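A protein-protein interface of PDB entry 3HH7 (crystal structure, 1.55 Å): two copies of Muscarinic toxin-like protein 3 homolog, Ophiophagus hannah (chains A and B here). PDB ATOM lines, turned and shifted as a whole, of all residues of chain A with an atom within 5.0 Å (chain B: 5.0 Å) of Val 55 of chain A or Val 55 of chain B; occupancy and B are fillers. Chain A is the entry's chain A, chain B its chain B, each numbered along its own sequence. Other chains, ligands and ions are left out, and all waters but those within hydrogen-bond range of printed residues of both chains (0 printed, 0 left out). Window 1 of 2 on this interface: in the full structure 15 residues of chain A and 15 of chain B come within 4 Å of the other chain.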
ATOM      1  N   LYS A  26     -27.039  -9.378  -3.097  1.00  0.00           N
ATOM      2  CA  LYS A  26     -28.377  -9.204  -3.633  1.00  0.00           C
ATOM      3  C   LYS A  26     -28.229  -9.080  -5.148  1.00  0.00           C
ATOM      4  O   LYS A  26     -27.463  -8.262  -5.636  1.00  0.00           O
ATOM      5  CB  LYS A  26     -29.048  -7.955  -3.051  1.00  0.00           C
ATOM      6  CG  LYS A  26     -30.475  -7.756  -3.481  1.00  0.00           C
ATOM      7  CD  LYS A  26     -31.017  -6.494  -2.863  1.00  0.00           C
ATOM      8  CE  LYS A  26     -32.507  -6.402  -3.047  1.00  0.00           C
ATOM      9  NZ  LYS A  26     -32.977  -5.044  -2.594  1.00  0.00           N
ATOM     10  N   SER A  27     -28.954  -9.918  -5.873  1.00  0.00           N
ATOM     11  CA  SER A  27     -28.880  -9.966  -7.327  1.00  0.00           C
ATOM     12  C   SER A  27     -30.282  -9.818  -7.898  1.00  0.00           C
ATOM     13  O   SER A  27     -31.163 -10.604  -7.556  1.00  0.00           O
ATOM     14  CB  SER A  27     -28.275 -11.307  -7.744  1.00  0.00           C
ATOM     15  OG  SER A  27     -28.237 -11.443  -9.149  1.00  0.00           O
ATOM     16  N   CYS A  45     -18.486 -12.463  -5.338  1.00  0.00           N
ATOM     17  CA  CYS A  45     -19.531 -11.553  -5.787  1.00  0.00           C
ATOM     18  C   CYS A  45     -20.044 -12.017  -7.149  1.00  0.00           C
ATOM     19  O   CYS A  45     -19.244 -12.171  -8.063  1.00  0.00           O
ATOM     20  CB  CYS A  45     -18.981 -10.128  -5.863  1.00  0.00           C
ATOM     21  SG  CYS A  45     -20.262  -8.904  -6.125  1.00  0.00           S
ATOM     22  N   PRO A  46     -21.363 -12.264  -7.288  1.00  0.00           N
ATOM     23  CA  PRO A  46     -21.875 -12.806  -8.559  1.00  0.00           C
ATOM     24  C   PRO A  46     -21.592 -11.904  -9.758  1.00  0.00           C
ATOM     25  O   PRO A  46     -21.598 -10.694  -9.631  1.00  0.00           O
ATOM     26  CB  PRO A  46     -23.397 -12.925  -8.323  1.00  0.00           C
ATOM     27  CG  PRO A  46     -23.565 -12.932  -6.862  1.00  0.00           C
ATOM     28  CD  PRO A  46     -22.437 -12.107  -6.288  1.00  0.00           C
ATOM     29  N   GLU A  47     -21.329 -12.507 -10.915  1.00  0.00           N
ATOM     30  CA  GLU A  47     -21.261 -11.758 -12.154  1.00  0.00           C
ATOM     31  C   GLU A  47     -22.609 -11.086 -12.452  1.00  0.00           C
ATOM     32  O   GLU A  47     -23.675 -11.610 -12.090  1.00  0.00           O
ATOM     33  CB  GLU A  47     -20.875 -12.690 -13.308  1.00  0.00           C
ATOM     34  CG  GLU A  47     -20.710 -12.012 -14.652  1.00  0.00           C
ATOM     35  CD  GLU A  47     -19.655 -10.928 -14.625  1.00  0.00           C
ATOM     36  OE1 GLU A  47     -18.498 -11.212 -14.991  1.00  0.00           O
ATOM     37  OE2 GLU A  47     -19.951  -9.770 -14.228  1.00  0.00           O
ATOM     38  N   LEU A  48     -22.554  -9.921 -13.094  1.00  0.00           N
ATOM     39  CA  LEU A  48     -23.762  -9.322 -13.630  1.00  0.00           C
ATOM     40  C   LEU A  48     -23.938  -9.807 -15.068  1.00  0.00           C
ATOM     41  O   LEU A  48     -23.212  -9.392 -15.973  1.00  0.00           O
ATOM     42  CB  LEU A  48     -23.736  -7.784 -13.560  1.00  0.00           C
ATOM     43  CG  LEU A  48     -25.017  -7.112 -14.066  1.00  0.00           C
ATOM     44  CD1 LEU A  48     -26.161  -7.421 -13.114  1.00  0.00           C
ATOM     45  CD2 LEU A  48     -24.835  -5.597 -14.226  1.00  0.00           C
ATOM     46  N   LYS A  53     -30.160  -6.785 -13.719  1.00  0.00           N
ATOM     47  CA  LYS A  53     -30.358  -5.350 -13.465  1.00  0.00           C
ATOM     48  C   LYS A  53     -29.209  -4.831 -12.597  1.00  0.00           C
ATOM     49  O   LYS A  53     -28.565  -3.824 -12.918  1.00  0.00           O
ATOM     50  CB  LYS A  53     -31.708  -5.085 -12.792  1.00  0.00           C
ATOM     51  CG  LYS A  53     -32.923  -5.274 -13.717  1.00  0.00           C
ATOM     52  CD  LYS A  53     -34.028  -4.274 -13.351  1.00  0.00           C
ATOM     53  CE  LYS A  53     -35.456  -4.734 -13.703  1.00  0.00           C
ATOM     54  NZ  LYS A  53     -36.193  -5.446 -12.574  1.00  0.00           N
ATOM     55  N   TYR A  54     -28.945  -5.526 -11.492  1.00  0.00           N
ATOM     56  CA  TYR A  54     -27.814  -5.179 -10.644  1.00  0.00           C
ATOM     57  C   TYR A  54     -27.377  -6.355  -9.808  1.00  0.00           C
ATOM     58  O   TYR A  54     -28.125  -7.325  -9.628  1.00  0.00           O
ATOM     59  CB  TYR A  54     -28.133  -3.949  -9.744  1.00  0.00           C
ATOM     60  CG  TYR A  54     -29.190  -4.195  -8.693  1.00  0.00           C
ATOM     61  CD1 TYR A  54     -28.891  -4.884  -7.521  1.00  0.00           C
ATOM     62  CD2 TYR A  54     -30.482  -3.716  -8.867  1.00  0.00           C
ATOM     63  CE1 TYR A  54     -29.865  -5.128  -6.543  1.00  0.00           C
ATOM     64  CE2 TYR A  54     -31.461  -3.929  -7.896  1.00  0.00           C
ATOM     65  CZ  TYR A  54     -31.143  -4.634  -6.740  1.00  0.00           C
ATOM     66  OH  TYR A  54     -32.117  -4.876  -5.794  1.00  0.00           O
ATOM     67  N   VAL A  55     -26.134  -6.261  -9.336  1.00  0.00           N
ATOM     68  CA  VAL A  55     -25.602  -7.131  -8.309  1.00  0.00           C
ATOM     69  C   VAL A  55     -25.005  -6.212  -7.237  1.00  0.00           C
ATOM     70  O   VAL A  55     -24.312  -5.234  -7.553  1.00  0.00           O
ATOM     71  CB  VAL A  55     -24.480  -8.062  -8.844  1.00  0.00           C
ATOM     72  CG1 VAL A  55     -23.783  -8.786  -7.690  1.00  0.00           C
ATOM     73  CG2 VAL A  55     -25.059  -9.116  -9.773  1.00  0.00           C
ATOM     74  N   TYR A  56     -25.288  -6.526  -5.978  1.00  0.00           N
ATOM     75  CA  TYR A  56     -24.753  -5.775  -4.859  1.00  0.00           C
ATOM     76  C   TYR A  56     -24.152  -6.736  -3.864  1.00  0.00           C
ATOM     77  O   TYR A  56     -24.822  -7.700  -3.455  1.00  0.00           O
ATOM     78  CB  TYR A  56     -25.873  -4.959  -4.195  1.00  0.00           C
ATOM     79  CG  TYR A  56     -25.428  -4.128  -3.010  1.00  0.00           C
ATOM     80  CD1 TYR A  56     -24.400  -3.190  -3.126  1.00  0.00           C
ATOM     81  CD2 TYR A  56     -26.056  -4.271  -1.787  1.00  0.00           C
ATOM     82  CE1 TYR A  56     -23.996  -2.413  -2.028  1.00  0.00           C
ATOM     83  CE2 TYR A  56     -25.673  -3.513  -0.692  1.00  0.00           C
ATOM     84  CZ  TYR A  56     -24.658  -2.581  -0.820  1.00  0.00           C
ATOM     85  OH  TYR A  56     -24.303  -1.837   0.295  1.00  0.00           O
ATOM     86  N   CYS A  57     -22.895  -6.495  -3.493  1.00  0.00           N
ATOM     87  CA  CYS A  57     -22.151  -7.349  -2.573  1.00  0.00           C
ATOM     88  C   CYS A  57     -21.661  -6.482  -1.436  1.00  0.00           C
ATOM     89  O   CYS A  57     -21.073  -5.442  -1.676  1.00  0.00           O
ATOM     90  CB  CYS A  57     -20.965  -8.035  -3.274  1.00  0.00           C
ATOM     91  SG  CYS A  57     -21.525  -9.161  -4.560  1.00  0.00           S
ATOM     92  N   LYS B  26     -19.516   0.529  -8.930  1.00  0.00           N
ATOM     93  CA  LYS B  26     -19.065   1.357  -7.829  1.00  0.00           C
ATOM     94  C   LYS B  26     -18.503   0.395  -6.802  1.00  0.00           C
ATOM     95  O   LYS B  26     -19.187  -0.548  -6.381  1.00  0.00           O
ATOM     96  CB  LYS B  26     -20.228   2.152  -7.246  1.00  0.00           C
ATOM     97  CG  LYS B  26     -19.858   3.046  -6.080  1.00  0.00           C
ATOM     98  CD  LYS B  26     -21.116   3.712  -5.582  1.00  0.00           C
ATOM     99  CE  LYS B  26     -20.780   4.817  -4.592  1.00  0.00           C
ATOM    100  NZ  LYS B  26     -22.049   5.327  -3.977  1.00  0.00           N
ATOM    101  N   SER B  27     -17.245   0.622  -6.428  1.00  0.00           N
ATOM    102  CA  SER B  27     -16.520  -0.254  -5.518  1.00  0.00           C
ATOM    103  C   SER B  27     -15.917   0.586  -4.398  1.00  0.00           C
ATOM    104  O   SER B  27     -15.200   1.551  -4.660  1.00  0.00           O
ATOM    105  CB  SER B  27     -15.402  -0.962  -6.285  1.00  0.00           C
ATOM    106  OG  SER B  27     -14.655  -1.817  -5.461  1.00  0.00           O
ATOM    107  N   CYS B  45     -18.293  -7.712 -13.435  1.00  0.00           N
ATOM    108  CA  CYS B  45     -18.417  -7.166 -12.088  1.00  0.00           C
ATOM    109  C   CYS B  45     -17.190  -7.562 -11.254  1.00  0.00           C
ATOM    110  O   CYS B  45     -16.873  -8.747 -11.169  1.00  0.00           O
ATOM    111  CB  CYS B  45     -19.713  -7.661 -11.441  1.00  0.00           C
ATOM    112  SG  CYS B  45     -20.171  -6.792  -9.905  1.00  0.00           S
ATOM    113  N   PRO B  46     -16.497  -6.580 -10.635  1.00  0.00           N
ATOM    114  CA  PRO B  46     -15.276  -6.966  -9.893  1.00  0.00           C
ATOM    115  C   PRO B  46     -15.556  -7.822  -8.662  1.00  0.00           C
ATOM    116  O   PRO B  46     -16.648  -7.745  -8.088  1.00  0.00           O
ATOM    117  CB  PRO B  46     -14.667  -5.618  -9.480  1.00  0.00           C
ATOM    118  CG  PRO B  46     -15.859  -4.692  -9.422  1.00  0.00           C
ATOM    119  CD  PRO B  46     -16.741  -5.124 -10.571  1.00  0.00           C
ATOM    120  N   GLU B  47     -14.585  -8.650  -8.284  1.00  0.00           N
ATOM    121  CA  GLU B  47     -14.649  -9.397  -7.033  1.00  0.00           C
ATOM    122  C   GLU B  47     -14.656  -8.424  -5.844  1.00  0.00           C
ATOM    123  O   GLU B  47     -14.065  -7.336  -5.911  1.00  0.00           O
ATOM    124  CB  GLU B  47     -13.446 -10.346  -6.938  1.00  0.00           C
ATOM    125  CG  GLU B  47     -13.483 -11.340  -5.770  1.00  0.00           C
ATOM    126  CD  GLU B  47     -14.782 -12.131  -5.759  1.00  0.00           C
ATOM    127  OE1 GLU B  47     -14.781 -13.251  -6.302  1.00  0.00           O
ATOM    128  OE2 GLU B  47     -15.811 -11.605  -5.257  1.00  0.00           O
ATOM    129  N   LEU B  48     -15.337  -8.815  -4.766  1.00  0.00           N
ATOM    130  CA  LEU B  48     -15.253  -8.076  -3.501  1.00  0.00           C
ATOM    131  C   LEU B  48     -14.039  -8.622  -2.758  1.00  0.00           C
ATOM    132  O   LEU B  48     -14.046  -9.782  -2.333  1.00  0.00           O
ATOM    133  CB  LEU B  48     -16.543  -8.213  -2.674  1.00  0.00           C
ATOM    134  CG  LEU B  48     -16.547  -7.388  -1.369  1.00  0.00           C
ATOM    135  CD1 LEU B  48     -16.466  -5.923  -1.658  1.00  0.00           C
ATOM    136  CD2 LEU B  48     -17.773  -7.671  -0.515  1.00  0.00           C
ATOM    137  N   LYS B  53     -15.532  -3.009   1.088  1.00  0.00           N
ATOM    138  CA  LYS B  53     -16.750  -2.813   1.865  1.00  0.00           C
ATOM    139  C   LYS B  53     -17.971  -3.255   1.052  1.00  0.00           C
ATOM    140  O   LYS B  53     -18.869  -3.944   1.548  1.00  0.00           O
ATOM    141  CB  LYS B  53     -16.902  -1.339   2.265  1.00  0.00           C
ATOM    142  CG  LYS B  53     -15.875  -0.884   3.296  1.00  0.00           C
ATOM    143  CD  LYS B  53     -16.249   0.463   3.892  1.00  0.00           C
ATOM    144  CE  LYS B  53     -15.638   1.609   3.103  1.00  0.00           C
ATOM    145  NZ  LYS B  53     -15.948   2.939   3.736  1.00  0.00           N
ATOM    146  N   TYR B  54     -17.991  -2.850  -0.215  1.00  0.00           N
ATOM    147  CA  TYR B  54     -19.050  -3.278  -1.119  1.00  0.00           C
ATOM    148  C   TYR B  54     -18.629  -3.117  -2.565  1.00  0.00           C
ATOM    149  O   TYR B  54     -17.727  -2.332  -2.886  1.00  0.00           O
ATOM    150  CB  TYR B  54     -20.366  -2.533  -0.861  1.00  0.00           C
ATOM    151  CG  TYR B  54     -20.341  -1.049  -1.127  1.00  0.00           C
ATOM    152  CD1 TYR B  54     -20.417  -0.552  -2.428  1.00  0.00           C
ATOM    153  CD2 TYR B  54     -20.298  -0.138  -0.072  1.00  0.00           C
ATOM    154  CE1 TYR B  54     -20.414   0.825  -2.674  1.00  0.00           C
ATOM    155  CE2 TYR B  54     -20.287   1.240  -0.310  1.00  0.00           C
ATOM    156  CZ  TYR B  54     -20.353   1.704  -1.615  1.00  0.00           C
ATOM    157  OH  TYR B  54     -20.342   3.064  -1.864  1.00  0.00           O
ATOM    158  N   VAL B  55     -19.325  -3.854  -3.419  1.00  0.00           N
ATOM    159  CA  VAL B  55     -19.247  -3.723  -4.871  1.00  0.00           C
ATOM    160  C   VAL B  55     -20.686  -3.648  -5.363  1.00  0.00           C
ATOM    161  O   VAL B  55     -21.545  -4.444  -4.947  1.00  0.00           O
ATOM    162  CB  VAL B  55     -18.579  -4.941  -5.510  1.00  0.00           C
ATOM    163  CG1 VAL B  55     -18.770  -4.935  -6.999  1.00  0.00           C
ATOM    164  CG2 VAL B  55     -17.086  -4.977  -5.190  1.00  0.00           C
ATOM    165  N   TYR B  56     -20.949  -2.686  -6.226  1.00  0.00           N
ATOM    166  CA  TYR B  56     -22.270  -2.536  -6.831  1.00  0.00           C
ATOM    167  C   TYR B  56     -22.077  -2.460  -8.331  1.00  0.00           C
ATOM    168  O   TYR B  56     -21.334  -1.604  -8.834  1.00  0.00           O
ATOM    169  CB  TYR B  56     -22.937  -1.261  -6.308  1.00  0.00           C
ATOM    170  CG  TYR B  56     -24.328  -0.973  -6.832  1.00  0.00           C
ATOM    171  CD1 TYR B  56     -25.335  -1.934  -6.759  1.00  0.00           C
ATOM    172  CD2 TYR B  56     -24.646   0.280  -7.355  1.00  0.00           C
ATOM    173  CE1 TYR B  56     -26.625  -1.644  -7.219  1.00  0.00           C
ATOM    174  CE2 TYR B  56     -25.921   0.578  -7.810  1.00  0.00           C
ATOM    175  CZ  TYR B  56     -26.898  -0.390  -7.750  1.00  0.00           C
ATOM    176  OH  TYR B  56     -28.169  -0.048  -8.201  1.00  0.00           O
ATOM    177  N   CYS B  57     -22.760  -3.352  -9.035  1.00  0.00           N
ATOM    178  CA  CYS B  57     -22.734  -3.385 -10.494  1.00  0.00           C
ATOM    179  C   CYS B  57     -24.140  -3.199 -11.005  1.00  0.00           C
ATOM    180  O   CYS B  57     -25.051  -3.856 -10.528  1.00  0.00           O
ATOM    181  CB  CYS B  57     -22.168  -4.725 -10.956  1.00  0.00           C
ATOM    182  SG  CYS B  57     -20.424  -4.859 -10.515  1.00  0.00           S
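Of the printed residues of chain B, Glu 47 of chain A touches Cys 45 (2.8 Å). Printed residues of chain B within 4 Å of Tyr 54 of chain A: Tyr 56 (3.7 Å) and Cys 57 (3.1 Å). Printed residues of chain B within 4 Å of Tyr 56 of chain A: Tyr 54 (3.8 Å), Val 55 (3.5 Å) and Tyr 56 (3.96 Å). Lys 26 of chain B touches none of the printed residues of chain A. Pro 46 of chain B touches none of the printed residues of chain A. Of chain A, only Val 55 (3.9 Å), Tyr 56 (3.5 Å) and Cys 57 (2.9 Å) come within 4 Å of Val 55 of chain B. The nearest residue of chain B that does not touch Val 55 of chain A is Cys 45 of chain B (4.6 Å). The nearest residue of chain A that does not touch Val 55 of chain B is Cys 45 of chain A (4.3 Å). The nearest printed residue of chain A that does not touch Cys 57 of chain B is Leu 48 of chain A (4.1 Å).
Of the 11 printed residues of chain A, 7 touch a printed residue of chain B. Printed residues of chain A that touch a printed residue of chain B: Cys 45, Glu 47, Leu 48, Tyr 54, Val 55, Tyr 56 and Cys 57. Hydrophobic or aromatic side chains of chain A that line the printed part of chain B: Tyr 54 and Tyr 56. Printed residues of chain B that touch a printed residue of chain A: Cys 45, Glu 47, Tyr 54, Val 55, Tyr 56 and Cys 57. Hydrophobic or aromatic side chains of chain B within 4 Å of the printed part of chain A: Tyr 54 and Tyr 56.
Among the printed residues, merely in contact across the chains: Cys 57 of chain A with Tyr 54 of chain B, Tyr 54 of chain A with Cys 57 of chain B, Val 55 of chain A with Tyr 56 of chain B, Tyr 56 of chain A with Val 55 of chain B, Tyr 54 of chain A with Tyr 56 of chain B, Tyr 56 of chain A with Tyr 54 of chain B, Val 55 of chain A with Val 55 of chain B, Tyr 56 of chain A with Tyr 56 of chain B and Leu 48 of chain A with Cys 45 of chain B.
The side-chain carboxylate (OE2) of Glu 47 of chain B sits at hydrogen-bond distance from the backbone NH (N) of Cys 45 of chain A, at 2.8 Å. The backbone carbonyl oxygen of Val 55 of chain B lies within hydrogen-bond range of the backbone NH of Cys 57 of chain A, 2.9 Å away. N of Cys 45 of chain B lies within hydrogen-bond range of OE2 of Glu 47 of chain A, at 2.8 Å. The backbone carbonyl oxygen of Val 55 of chain A is in hydrogen-bond range of the backbone NH of Cys 57 of chain B (2.9 Å).
The side-chain amino group (NZ) of Lys 26 of chain A lies close to the side-chain hydroxyl (OH) of Tyr 54 of chain A (3.3 Å). The backbone carbonyl oxygen (O) of Lys 26 of chain A sits at hydrogen-bond distance from the backbone NH (N) of Tyr 56 of chain A (2.8 Å). The side-chain sulfur (SG) of Cys 57 of chain A is disulfide-bonded to the side-chain sulfur (SG) of Cys 45 of chain A. The backbone carbonyl oxygen (O) of Lys 26 of chain B lies within hydrogen-bond range of the backbone NH (N) of Tyr 56 of chain B (2.8 Å). SG of Cys 45 of chain B forms a disulfide with SG of Cys 57 of chain B (2.0 Å).
Tyr 54 of chain A touches Tyr 56 of chain B, and with the chains exchanged Tyr 56 of chain A touches Tyr 54 of chain B. Tyr 54 of chain A touches Cys 57 of chain B, and with the chains exchanged Cys 57 of chain A touches Tyr 54 of chain B. Val 55 of chain A touches Cys 57 of chain B, and with the chains exchanged Cys 57 of chain A touches Val 55 of chain B. Tyr 56 of chain A touches its own counterpart, Tyr 56 of chain B. Positions printed for both chains: 26, 27, 45, 46, 47, 48, 53, 54, 55, 56 and 57. Of the 13 pairs that touch across the chains among the printed residues, 12 have their exchanged pair printed and touching as well.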
